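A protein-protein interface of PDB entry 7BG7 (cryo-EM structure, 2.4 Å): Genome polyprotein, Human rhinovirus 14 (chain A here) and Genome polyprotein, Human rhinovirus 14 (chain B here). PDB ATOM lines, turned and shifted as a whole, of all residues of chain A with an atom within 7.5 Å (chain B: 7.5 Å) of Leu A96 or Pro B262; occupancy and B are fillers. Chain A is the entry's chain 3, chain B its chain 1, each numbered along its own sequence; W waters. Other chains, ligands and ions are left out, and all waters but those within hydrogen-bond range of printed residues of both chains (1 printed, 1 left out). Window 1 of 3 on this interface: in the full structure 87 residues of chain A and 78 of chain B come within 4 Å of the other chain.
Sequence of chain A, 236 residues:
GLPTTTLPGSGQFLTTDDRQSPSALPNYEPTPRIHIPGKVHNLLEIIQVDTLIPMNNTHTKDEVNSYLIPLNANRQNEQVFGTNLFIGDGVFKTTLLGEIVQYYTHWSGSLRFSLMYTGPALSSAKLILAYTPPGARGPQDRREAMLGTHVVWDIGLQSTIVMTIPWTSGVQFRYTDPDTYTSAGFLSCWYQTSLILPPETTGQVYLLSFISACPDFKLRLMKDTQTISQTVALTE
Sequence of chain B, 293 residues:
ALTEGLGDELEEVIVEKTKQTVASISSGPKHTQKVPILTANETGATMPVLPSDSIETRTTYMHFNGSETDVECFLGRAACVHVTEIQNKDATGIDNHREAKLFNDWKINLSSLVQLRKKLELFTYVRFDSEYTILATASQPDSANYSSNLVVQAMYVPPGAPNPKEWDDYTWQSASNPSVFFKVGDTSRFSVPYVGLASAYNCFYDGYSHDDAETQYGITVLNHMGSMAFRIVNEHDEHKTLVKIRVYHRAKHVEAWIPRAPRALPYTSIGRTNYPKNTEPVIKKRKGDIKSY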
ATOM      1  N   LEU A  43     -13.776   9.643  -5.392  1.00  0.00           N
ATOM      2  CA  LEU A  43     -12.579   8.898  -5.039  1.00  0.00           C
ATOM      3  C   LEU A  43     -11.329   9.724  -5.275  1.00  0.00           C
ATOM      4  O   LEU A  43     -10.257   9.360  -4.786  1.00  0.00           O
ATOM      5  CB  LEU A  43     -12.519   7.593  -5.817  1.00  0.00           C
ATOM      6  CG  LEU A  43     -12.910   6.388  -4.966  1.00  0.00           C
ATOM      7  CD1 LEU A  43     -14.368   6.446  -4.588  1.00  0.00           C
ATOM      8  CD2 LEU A  43     -12.623   5.134  -5.740  1.00  0.00           C
ATOM      9  N   GLU A  45     -10.939  12.395  -3.956  1.00  0.00           N
ATOM     10  CA  GLU A  45     -10.736  13.068  -2.680  1.00  0.00           C
ATOM     11  C   GLU A  45      -9.813  12.260  -1.785  1.00  0.00           C
ATOM     12  O   GLU A  45      -9.052  12.838  -1.005  1.00  0.00           O
ATOM     13  CB  GLU A  45     -12.064  13.290  -1.954  1.00  0.00           C
ATOM     14  CG  GLU A  45     -13.022  14.248  -2.626  1.00  0.00           C
ATOM     15  CD  GLU A  45     -14.390  14.242  -1.960  1.00  0.00           C
ATOM     16  OE1 GLU A  45     -14.897  13.147  -1.645  1.00  0.00           O
ATOM     17  OE2 GLU A  45     -14.953  15.331  -1.735  1.00  0.00           O
ATOM     18  N   ILE A  46      -9.886  10.933  -1.863  1.00  0.00           N
ATOM     19  CA  ILE A  46      -9.223  10.076  -0.892  1.00  0.00           C
ATOM     20  C   ILE A  46      -7.852   9.649  -1.403  1.00  0.00           C
ATOM     21  O   ILE A  46      -6.975   9.329  -0.587  1.00  0.00           O
ATOM     22  CB  ILE A  46     -10.080   8.845  -0.521  1.00  0.00           C
ATOM     23  CG1 ILE A  46     -10.244   7.892  -1.702  1.00  0.00           C
ATOM     24  CG2 ILE A  46     -11.445   9.289  -0.027  1.00  0.00           C
ATOM     25  CD1 ILE A  46     -10.943   6.602  -1.331  1.00  0.00           C
ATOM     26  N   ILE A  47      -7.637   9.646  -2.721  1.00  0.00           N
ATOM     27  CA  ILE A  47      -6.331   9.294  -3.266  1.00  0.00           C
ATOM     28  C   ILE A  47      -5.306  10.367  -2.957  1.00  0.00           C
ATOM     29  O   ILE A  47      -4.110  10.154  -3.166  1.00  0.00           O
ATOM     30  CB  ILE A  47      -6.367   9.069  -4.791  1.00  0.00           C
ATOM     31  CG1 ILE A  47      -7.021  10.258  -5.487  1.00  0.00           C
ATOM     32  CG2 ILE A  47      -7.070   7.780  -5.118  1.00  0.00           C
ATOM     33  CD1 ILE A  47      -6.817  10.277  -6.977  1.00  0.00           C
ATOM     34  N   GLN A  48      -5.759  11.528  -2.504  1.00  0.00           N
ATOM     35  CA  GLN A  48      -4.889  12.637  -2.161  1.00  0.00           C
ATOM     36  C   GLN A  48      -4.323  12.508  -0.755  1.00  0.00           C
ATOM     37  O   GLN A  48      -3.565  13.381  -0.327  1.00  0.00           O
ATOM     38  CB  GLN A  48      -5.644  13.953  -2.285  1.00  0.00           C
ATOM     39  CG  GLN A  48      -5.979  14.323  -3.704  1.00  0.00           C
ATOM     40  CD  GLN A  48      -6.629  15.678  -3.804  1.00  0.00           C
ATOM     41  OE1 GLN A  48      -6.185  16.634  -3.180  1.00  0.00           O
ATOM     42  NE2 GLN A  48      -7.712  15.761  -4.566  1.00  0.00           N
ATOM     43  N   VAL A  49      -4.668  11.445  -0.043  1.00  0.00           N
ATOM     44  CA  VAL A  49      -4.150  11.173   1.291  1.00  0.00           C
ATOM     45  C   VAL A  49      -2.919  10.290   1.154  1.00  0.00           C
ATOM     46  O   VAL A  49      -2.960   9.266   0.468  1.00  0.00           O
ATOM     47  CB  VAL A  49      -5.218  10.493   2.165  1.00  0.00           C
ATOM     48  CG1 VAL A  49      -4.692  10.254   3.568  1.00  0.00           C
ATOM     49  CG2 VAL A  49      -6.484  11.328   2.206  1.00  0.00           C
ATOM     50  N   ASP A  50      -1.815  10.694   1.785  1.00  0.00           N
ATOM     51  CA  ASP A  50      -0.587   9.905   1.729  1.00  0.00           C
ATOM     52  C   ASP A  50      -0.750   8.579   2.456  1.00  0.00           C
ATOM     53  O   ASP A  50      -1.250   8.531   3.582  1.00  0.00           O
ATOM     54  CB  ASP A  50       0.586  10.656   2.356  1.00  0.00           C
ATOM     55  CG  ASP A  50       1.117  11.758   1.482  1.00  0.00           C
ATOM     56  OD1 ASP A  50       2.018  11.491   0.659  1.00  0.00           O
ATOM     57  OD2 ASP A  50       0.693  12.909   1.666  1.00  0.00           O
ATOM     58  N   THR A  51      -0.285   7.508   1.822  1.00  0.00           N
ATOM     59  CA  THR A  51      -0.138   6.213   2.463  1.00  0.00           C
ATOM     60  C   THR A  51       1.268   5.694   2.199  1.00  0.00           C
ATOM     61  O   THR A  51       1.927   6.086   1.236  1.00  0.00           O
ATOM     62  CB  THR A  51      -1.171   5.180   1.970  1.00  0.00           C
ATOM     63  OG1 THR A  51      -0.961   4.900   0.584  1.00  0.00           O
ATOM     64  CG2 THR A  51      -2.592   5.681   2.194  1.00  0.00           C
ATOM     65  N   LEU A  52       1.719   4.804   3.075  1.00  0.00           N
ATOM     66  CA  LEU A  52       3.085   4.312   3.027  1.00  0.00           C
ATOM     67  C   LEU A  52       3.298   3.445   1.793  1.00  0.00           C
ATOM     68  O   LEU A  52       2.399   2.740   1.340  1.00  0.00           O
ATOM     69  CB  LEU A  52       3.397   3.502   4.284  1.00  0.00           C
ATOM     70  CG  LEU A  52       3.501   4.309   5.576  1.00  0.00           C
ATOM     71  CD1 LEU A  52       3.480   3.378   6.770  1.00  0.00           C
ATOM     72  CD2 LEU A  52       4.749   5.174   5.588  1.00  0.00           C
ATOM     73  N   PHE A  92       3.838   0.037  -5.755  1.00  0.00           N
ATOM     74  CA  PHE A  92       2.668   0.876  -5.583  1.00  0.00           C
ATOM     75  C   PHE A  92       1.384   0.074  -5.586  1.00  0.00           C
ATOM     76  O   PHE A  92       0.340   0.606  -5.208  1.00  0.00           O
ATOM     77  CB  PHE A  92       2.593   1.923  -6.694  1.00  0.00           C
ATOM     78  CG  PHE A  92       3.808   2.771  -6.808  1.00  0.00           C
ATOM     79  CD1 PHE A  92       4.034   3.794  -5.910  1.00  0.00           C
ATOM     80  CD2 PHE A  92       4.719   2.561  -7.824  1.00  0.00           C
ATOM     81  CE1 PHE A  92       5.149   4.581  -6.018  1.00  0.00           C
ATOM     82  CE2 PHE A  92       5.828   3.349  -7.937  1.00  0.00           C
ATOM     83  CZ  PHE A  92       6.047   4.360  -7.036  1.00  0.00           C
ATOM     84  N   LYS A  93       1.450  -1.202  -5.961  1.00  0.00           N
ATOM     85  CA  LYS A  93       0.241  -1.970  -6.211  1.00  0.00           C
ATOM     86  C   LYS A  93      -0.657  -2.018  -4.984  1.00  0.00           C
ATOM     87  O   LYS A  93      -1.883  -2.065  -5.121  1.00  0.00           O
ATOM     88  CB  LYS A  93       0.620  -3.373  -6.674  1.00  0.00           C
ATOM     89  CG  LYS A  93      -0.488  -4.106  -7.394  1.00  0.00           C
ATOM     90  CD  LYS A  93      -0.017  -5.461  -7.867  1.00  0.00           C
ATOM     91  CE  LYS A  93      -1.099  -6.198  -8.643  1.00  0.00           C
ATOM     92  NZ  LYS A  93      -1.323  -5.612  -9.986  1.00  0.00           N
ATOM     93  N   THR A  94      -0.078  -2.000  -3.784  1.00  0.00           N
ATOM     94  CA  THR A  94      -0.835  -2.228  -2.562  1.00  0.00           C
ATOM     95  C   THR A  94      -1.178  -0.937  -1.840  1.00  0.00           C
ATOM     96  O   THR A  94      -1.996  -0.960  -0.919  1.00  0.00           O
ATOM     97  CB  THR A  94      -0.065  -3.140  -1.602  1.00  0.00           C
ATOM     98  OG1 THR A  94       1.214  -2.568  -1.317  1.00  0.00           O
ATOM     99  CG2 THR A  94       0.115  -4.511  -2.209  1.00  0.00           C
ATOM    100  N   THR A  95      -0.568   0.175  -2.224  1.00  0.00           N
ATOM    101  CA  THR A  95      -0.860   1.450  -1.602  1.00  0.00           C
ATOM    102  C   THR A  95      -2.278   1.872  -1.954  1.00  0.00           C
ATOM    103  O   THR A  95      -2.884   1.369  -2.902  1.00  0.00           O
ATOM    104  CB  THR A  95       0.137   2.522  -2.043  1.00  0.00           C
ATOM    105  OG1 THR A  95       0.008   2.751  -3.448  1.00  0.00           O
ATOM    106  CG2 THR A  95       1.555   2.102  -1.731  1.00  0.00           C
ATOM    107  N   LEU A  96      -2.808   2.815  -1.178  1.00  0.00           N
ATOM    108  CA  LEU A  96      -4.157   3.299  -1.446  1.00  0.00           C
ATOM    109  C   LEU A  96      -4.248   3.858  -2.853  1.00  0.00           C
ATOM    110  O   LEU A  96      -5.206   3.573  -3.581  1.00  0.00           O
ATOM    111  CB  LEU A  96      -4.556   4.357  -0.420  1.00  0.00           C
ATOM    112  CG  LEU A  96      -5.930   4.988  -0.651  1.00  0.00           C
ATOM    113  CD1 LEU A  96      -7.028   3.956  -0.551  1.00  0.00           C
ATOM    114  CD2 LEU A  96      -6.166   6.110   0.336  1.00  0.00           C
ATOM    115  N   LEU A  97      -3.255   4.646  -3.261  1.00  0.00           N
ATOM    116  CA  LEU A  97      -3.273   5.192  -4.608  1.00  0.00           C
ATOM    117  C   LEU A  97      -3.311   4.060  -5.621  1.00  0.00           C
ATOM    118  O   LEU A  97      -4.150   4.058  -6.523  1.00  0.00           O
ATOM    119  CB  LEU A  97      -2.069   6.103  -4.831  1.00  0.00           C
ATOM    120  CG  LEU A  97      -2.050   6.859  -6.160  1.00  0.00           C
ATOM    121  CD1 LEU A  97      -1.436   8.224  -5.988  1.00  0.00           C
ATOM    122  CD2 LEU A  97      -1.268   6.081  -7.197  1.00  0.00           C
ATOM    123  N   GLY A  98      -2.412   3.084  -5.484  1.00  0.00           N
ATOM    124  CA  GLY A  98      -2.380   1.974  -6.427  1.00  0.00           C
ATOM    125  C   GLY A  98      -3.674   1.179  -6.438  1.00  0.00           C
ATOM    126  O   GLY A  98      -4.124   0.721  -7.491  1.00  0.00           O
ATOM    127  N   GLU A  99      -4.287   1.001  -5.266  1.00  0.00           N
ATOM    128  CA  GLU A  99      -5.507   0.204  -5.174  1.00  0.00           C
ATOM    129  C   GLU A  99      -6.644   0.901  -5.895  1.00  0.00           C
ATOM    130  O   GLU A  99      -7.351   0.288  -6.699  1.00  0.00           O
ATOM    131  CB  GLU A  99      -5.881  -0.042  -3.711  1.00  0.00           C
ATOM    132  CG  GLU A  99      -4.956  -0.959  -2.941  1.00  0.00           C
ATOM    133  CD  GLU A  99      -4.844  -2.309  -3.605  1.00  0.00           C
ATOM    134  OE1 GLU A  99      -5.884  -2.795  -4.093  1.00  0.00           O
ATOM    135  OE2 GLU A  99      -3.743  -2.891  -3.639  1.00  0.00           O
ATOM    136  N   ILE A 100      -6.826   2.191  -5.626  1.00  0.00           N
ATOM    137  CA  ILE A 100      -7.872   2.924  -6.318  1.00  0.00           C
ATOM    138  C   ILE A 100      -7.546   3.026  -7.805  1.00  0.00           C
ATOM    139  O   ILE A 100      -8.451   3.027  -8.645  1.00  0.00           O
ATOM    140  CB  ILE A 100      -8.039   4.300  -5.657  1.00  0.00           C
ATOM    141  CG1 ILE A 100      -8.597   4.120  -4.240  1.00  0.00           C
ATOM    142  CG2 ILE A 100      -8.943   5.183  -6.495  1.00  0.00           C
ATOM    143  CD1 ILE A 100      -8.405   5.312  -3.343  1.00  0.00           C
ATOM    144  N   VAL A 101      -6.259   3.057  -8.157  1.00  0.00           N
ATOM    145  CA  VAL A 101      -5.840   3.208  -9.546  1.00  0.00           C
ATOM    146  C   VAL A 101      -6.143   1.946 -10.339  1.00  0.00           C
ATOM    147  O   VAL A 101      -6.421   2.011 -11.540  1.00  0.00           O
ATOM    148  CB  VAL A 101      -4.346   3.585  -9.600  1.00  0.00           C
ATOM    149  CG1 VAL A 101      -3.682   3.049 -10.846  1.00  0.00           C
ATOM    150  CG2 VAL A 101      -4.194   5.089  -9.539  1.00  0.00           C
ATOM    151  N   GLN A 102      -6.069   0.783  -9.700  1.00  0.00           N
ATOM    152  CA  GLN A 102      -6.286  -0.462 -10.420  1.00  0.00           C
ATOM    153  C   GLN A 102      -7.747  -0.654 -10.804  1.00  0.00           C
ATOM    154  O   GLN A 102      -8.051  -1.559 -11.583  1.00  0.00           O
ATOM    155  CB  GLN A 102      -5.785  -1.641  -9.593  1.00  0.00           C
ATOM    156  CG  GLN A 102      -4.280  -1.818  -9.678  1.00  0.00           C
ATOM    157  CD  GLN A 102      -3.767  -2.889  -8.750  1.00  0.00           C
ATOM    158  OE1 GLN A 102      -3.743  -4.065  -9.097  1.00  0.00           O
ATOM    159  NE2 GLN A 102      -3.353  -2.487  -7.559  1.00  0.00           N
ATOM    160  N   TYR A 103      -8.648   0.178 -10.296  1.00  0.00           N
ATOM    161  CA  TYR A 103     -10.054   0.119 -10.658  1.00  0.00           C
ATOM    162  C   TYR A 103     -10.347   0.904 -11.927  1.00  0.00           C
ATOM    163  O   TYR A 103     -11.483   0.884 -12.408  1.00  0.00           O
ATOM    164  CB  TYR A 103     -10.911   0.666  -9.519  1.00  0.00           C
ATOM    165  CG  TYR A 103     -11.180  -0.329  -8.433  1.00  0.00           C
ATOM    166  CD1 TYR A 103     -11.978  -1.436  -8.664  1.00  0.00           C
ATOM    167  CD2 TYR A 103     -10.628  -0.169  -7.174  1.00  0.00           C
ATOM    168  CE1 TYR A 103     -12.225  -2.345  -7.675  1.00  0.00           C
ATOM    169  CE2 TYR A 103     -10.870  -1.075  -6.181  1.00  0.00           C
ATOM    170  CZ  TYR A 103     -11.667  -2.163  -6.433  1.00  0.00           C
ATOM    171  OH  TYR A 103     -11.913  -3.071  -5.440  1.00  0.00           O
ATOM    172  N   ILE A 211       3.151   7.890  -0.736  1.00  0.00           N
ATOM    173  CA  ILE A 211       2.659   8.253  -2.056  1.00  0.00           C
ATOM    174  C   ILE A 211       1.257   8.822  -1.916  1.00  0.00           C
ATOM    175  O   ILE A 211       0.480   8.391  -1.059  1.00  0.00           O
ATOM    176  CB  ILE A 211       2.673   7.049  -3.024  1.00  0.00           C
ATOM    177  CG1 ILE A 211       2.380   7.497  -4.455  1.00  0.00           C
ATOM    178  CG2 ILE A 211       1.673   5.999  -2.595  1.00  0.00           C
ATOM    179  CD1 ILE A 211       3.389   8.445  -5.030  1.00  0.00           C
ATOM    180  N   THR A 227      -6.481  -7.417  -7.734  1.00  0.00           N
ATOM    181  CA  THR A 227      -5.885  -7.589  -6.412  1.00  0.00           C
ATOM    182  C   THR A 227      -6.542  -8.736  -5.657  1.00  0.00           C
ATOM    183  O   THR A 227      -5.867  -9.465  -4.922  1.00  0.00           O
ATOM    184  CB  THR A 227      -5.987  -6.298  -5.604  1.00  0.00           C
ATOM    185  OG1 THR A 227      -7.304  -5.748  -5.728  1.00  0.00           O
ATOM    186  CG2 THR A 227      -4.965  -5.287  -6.087  1.00  0.00           C
ATOM    187  N   LYS B 118     -15.070  -5.807  -1.986  1.00  0.00           N
ATOM    188  CA  LYS B 118     -13.906  -4.966  -1.730  1.00  0.00           C
ATOM    189  C   LYS B 118     -14.226  -3.509  -2.033  1.00  0.00           C
ATOM    190  O   LYS B 118     -13.901  -2.611  -1.237  1.00  0.00           O
ATOM    191  CB  LYS B 118     -12.712  -5.435  -2.561  1.00  0.00           C
ATOM    192  CG  LYS B 118     -11.480  -4.555  -2.379  1.00  0.00           C
ATOM    193  CD  LYS B 118     -10.266  -5.080  -3.116  1.00  0.00           C
ATOM    194  CE  LYS B 118      -9.123  -4.082  -3.037  1.00  0.00           C
ATOM    195  NZ  LYS B 118      -7.811  -4.669  -3.397  1.00  0.00           N
ATOM    196  N   GLU B 121     -16.281  -2.238   0.739  1.00  0.00           N
ATOM    197  CA  GLU B 121     -15.545  -2.250   1.985  1.00  0.00           C
ATOM    198  C   GLU B 121     -14.474  -1.179   1.983  1.00  0.00           C
ATOM    199  O   GLU B 121     -13.779  -1.008   2.985  1.00  0.00           O
ATOM    200  CB  GLU B 121     -14.912  -3.621   2.219  1.00  0.00           C
ATOM    201  CG  GLU B 121     -15.870  -4.671   2.728  1.00  0.00           C
ATOM    202  CD  GLU B 121     -15.152  -5.879   3.265  1.00  0.00           C
ATOM    203  OE1 GLU B 121     -15.797  -6.716   3.927  1.00  0.00           O
ATOM    204  OE2 GLU B 121     -13.933  -5.992   3.031  1.00  0.00           O
ATOM    205  N   LEU B 122     -14.353  -0.442   0.880  1.00  0.00           N
ATOM    206  CA  LEU B 122     -13.505   0.738   0.906  1.00  0.00           C
ATOM    207  C   LEU B 122     -14.096   1.810   1.809  1.00  0.00           C
ATOM    208  O   LEU B 122     -13.414   2.790   2.114  1.00  0.00           O
ATOM    209  CB  LEU B 122     -13.316   1.304  -0.498  1.00  0.00           C
ATOM    210  CG  LEU B 122     -12.249   0.667  -1.386  1.00  0.00           C
ATOM    211  CD1 LEU B 122     -12.284   1.286  -2.774  1.00  0.00           C
ATOM    212  CD2 LEU B 122     -10.868   0.824  -0.767  1.00  0.00           C
ATOM    213  N   PRO B 259     -13.702   6.602   4.612  1.00  0.00           N
ATOM    214  CA  PRO B 259     -12.879   5.731   3.771  1.00  0.00           C
ATOM    215  C   PRO B 259     -12.033   4.806   4.627  1.00  0.00           C
ATOM    216  O   PRO B 259     -11.696   5.112   5.770  1.00  0.00           O
ATOM    217  CB  PRO B 259     -12.005   6.710   2.983  1.00  0.00           C
ATOM    218  CG  PRO B 259     -12.036   7.957   3.766  1.00  0.00           C
ATOM    219  CD  PRO B 259     -13.371   8.018   4.403  1.00  0.00           C
ATOM    220  N   ARG B 260     -11.705   3.655   4.061  1.00  0.00           N
ATOM    221  CA  ARG B 260     -11.113   2.555   4.795  1.00  0.00           C
ATOM    222  C   ARG B 260      -9.927   1.995   4.019  1.00  0.00           C
ATOM    223  O   ARG B 260      -9.789   2.210   2.817  1.00  0.00           O
ATOM    224  CB  ARG B 260     -12.183   1.484   5.045  1.00  0.00           C
ATOM    225  CG  ARG B 260     -11.777   0.364   5.932  1.00  0.00           C
ATOM    226  CD  ARG B 260     -12.998  -0.357   6.477  1.00  0.00           C
ATOM    227  NE  ARG B 260     -13.668   0.436   7.496  1.00  0.00           N
ATOM    228  CZ  ARG B 260     -13.588   0.220   8.803  1.00  0.00           C
ATOM    229  NH1 ARG B 260     -12.871  -0.775   9.294  1.00  0.00           N
ATOM    230  NH2 ARG B 260     -14.231   1.016   9.630  1.00  0.00           N
ATOM    231  N   ALA B 261      -9.052   1.301   4.732  1.00  0.00           N
ATOM    232  CA  ALA B 261      -7.945   0.610   4.089  1.00  0.00           C
ATOM    233  C   ALA B 261      -8.471  -0.500   3.180  1.00  0.00           C
ATOM    234  O   ALA B 261      -9.328  -1.283   3.605  1.00  0.00           O
ATOM    235  CB  ALA B 261      -6.991   0.035   5.135  1.00  0.00           C
ATOM    236  N   PRO B 262      -8.024  -0.578   1.925  1.00  0.00           N
ATOM    237  CA  PRO B 262      -8.558  -1.603   1.019  1.00  0.00           C
ATOM    238  C   PRO B 262      -8.240  -3.010   1.492  1.00  0.00           C
ATOM    239  O   PRO B 262      -7.228  -3.256   2.150  1.00  0.00           O
ATOM    240  CB  PRO B 262      -7.860  -1.305  -0.312  1.00  0.00           C
ATOM    241  CG  PRO B 262      -7.373   0.074  -0.194  1.00  0.00           C
ATOM    242  CD  PRO B 262      -7.054   0.287   1.242  1.00  0.00           C
ATOM    243  N   ARG B 263      -9.099  -3.945   1.101  1.00  0.00           N
ATOM    244  CA  ARG B 263      -8.900  -5.346   1.439  1.00  0.00           C
ATOM    245  C   ARG B 263      -7.703  -5.909   0.691  1.00  0.00           C
ATOM    246  O   ARG B 263      -7.577  -5.736  -0.523  1.00  0.00           O
ATOM    247  CB  ARG B 263     -10.149  -6.157   1.102  1.00  0.00           C
ATOM    248  CG  ARG B 263     -10.060  -7.626   1.492  1.00  0.00           C
ATOM    249  CD  ARG B 263     -10.258  -7.808   2.973  1.00  0.00           C
ATOM    250  NE  ARG B 263     -10.122  -9.199   3.379  1.00  0.00           N
ATOM    251  CZ  ARG B 263     -10.494  -9.670   4.563  1.00  0.00           C
ATOM    252  NH1 ARG B 263     -11.033  -8.863   5.461  1.00  0.00           N
ATOM    253  NH2 ARG B 263     -10.333 -10.947   4.846  1.00  0.00           N
ATOM    254  N   ALA B 264      -6.822  -6.583   1.420  1.00  0.00           N
ATOM    255  CA  ALA B 264      -5.608  -7.141   0.851  1.00  0.00           C
ATOM    256  C   ALA B 264      -5.639  -8.653   0.757  1.00  0.00           C
ATOM    257  O   ALA B 264      -5.082  -9.214  -0.183  1.00  0.00           O
ATOM    258  CB  ALA B 264      -4.388  -6.724   1.681  1.00  0.00           C
ATOM    259  N   LEU B 265      -6.283  -9.316   1.699  1.00  0.00           N
ATOM    260  CA  LEU B 265      -6.275 -10.759   1.797  1.00  0.00           C
ATOM    261  C   LEU B 265      -7.609 -11.326   1.346  1.00  0.00           C
ATOM    262  O   LEU B 265      -8.629 -10.632   1.355  1.00  0.00           O
ATOM    263  CB  LEU B 265      -5.981 -11.199   3.236  1.00  0.00           C
ATOM    264  CG  LEU B 265      -4.580 -10.858   3.750  1.00  0.00           C
ATOM    265  CD1 LEU B 265      -4.392 -11.354   5.164  1.00  0.00           C
ATOM    266  CD2 LEU B 265      -3.521 -11.455   2.848  1.00  0.00           C
ATOM    267  N   TYR B 267     -11.177 -13.272   1.351  1.00  0.00           N
ATOM    268  CA  TYR B 267     -12.251 -13.392   2.320  1.00  0.00           C
ATOM    269  C   TYR B 267     -12.525 -14.864   2.585  1.00  0.00           C
ATOM    270  O   TYR B 267     -12.125 -15.742   1.821  1.00  0.00           O
ATOM    271  CB  TYR B 267     -13.528 -12.720   1.818  1.00  0.00           C
ATOM    272  CG  TYR B 267     -13.464 -11.223   1.631  1.00  0.00           C
ATOM    273  CD1 TYR B 267     -13.593 -10.355   2.711  1.00  0.00           C
ATOM    274  CD2 TYR B 267     -13.289 -10.679   0.373  1.00  0.00           C
ATOM    275  CE1 TYR B 267     -13.552  -8.991   2.533  1.00  0.00           C
ATOM    276  CE2 TYR B 267     -13.244  -9.328   0.188  1.00  0.00           C
ATOM    277  CZ  TYR B 267     -13.379  -8.484   1.264  1.00  0.00           C
ATOM    278  OH  TYR B 267     -13.334  -7.132   1.052  1.00  0.00           O
HETATM  279  O   HOH W   1      -4.169  -8.118  -3.331  1.00  0.00           O
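The side-chain amino group (NZ) of Lys B118 sits at hydrogen-bond distance from the side-chain hydroxyl (OG1) of Thr A227, at 2.6 Å. OE1 of Glu A99 lies within salt-bridge range of NZ of Lys B118 (2.8 Å).
Water W1 lies within hydrogen-bond range of O of Thr A227 and O of Ala B264.
O of Arg B263 lies within hydrogen-bond range of NZ of Lys B118. The backbone NH (N) of Leu A96 is in hydrogen-bond range of the side-chain hydroxyl (OG1) of Thr A51 (3.3 Å). The backbone carbonyl oxygen (O) of Lys A93 sits close to the side-chain carboxylate (OE2) of Glu A99 (2.5 Å).
CD1 of Leu A96 touches CG of Pro B262 (3.9 Å). Pro B262 touches Glu A99 (CG to CG, 3.8 Å). CG of Lys B118 touches OH of Tyr A103 (3.4 Å).
Leu A52 touches none of the printed residues of chain B. Of chain B, only Pro B262 (3.9 Å) comes within 4 Å of Leu A96. Printed residues of chain B within 4 Å of Glu A99: Lys B118 (2.8 Å) and Pro B262 (3.8 Å). Gln A102 touches none of the printed residues of chain B. Of the printed residues of chain B, Tyr A103 touches Lys B118. Of chain A, only Leu A96 and Glu A99 come within 4 Å of Pro B262. The nearest residue of chain A that does not touch Pro B262 is Thr A95 (5.4 Å). The nearest printed residue of chain B that does not touch Tyr A103 is Leu B122 (4.4 Å).
Of the 11 printed residues of chain B, 2 touch a printed residue of chain A. Hydrophobic or aromatic side chains of chain B that line the printed part of chain A: Pro B262. Along chain B the printed residues that touch a printed residue of chain A span positions 118 to 262. Among the printed residues, 5 pairs touch across the chains. Among the printed residues, Asp or Glu carboxylates within 4 Å of a Lys or Arg side-chain nitrogen of the other chain: Glu A99 with Lys B118 (2.8 Å).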
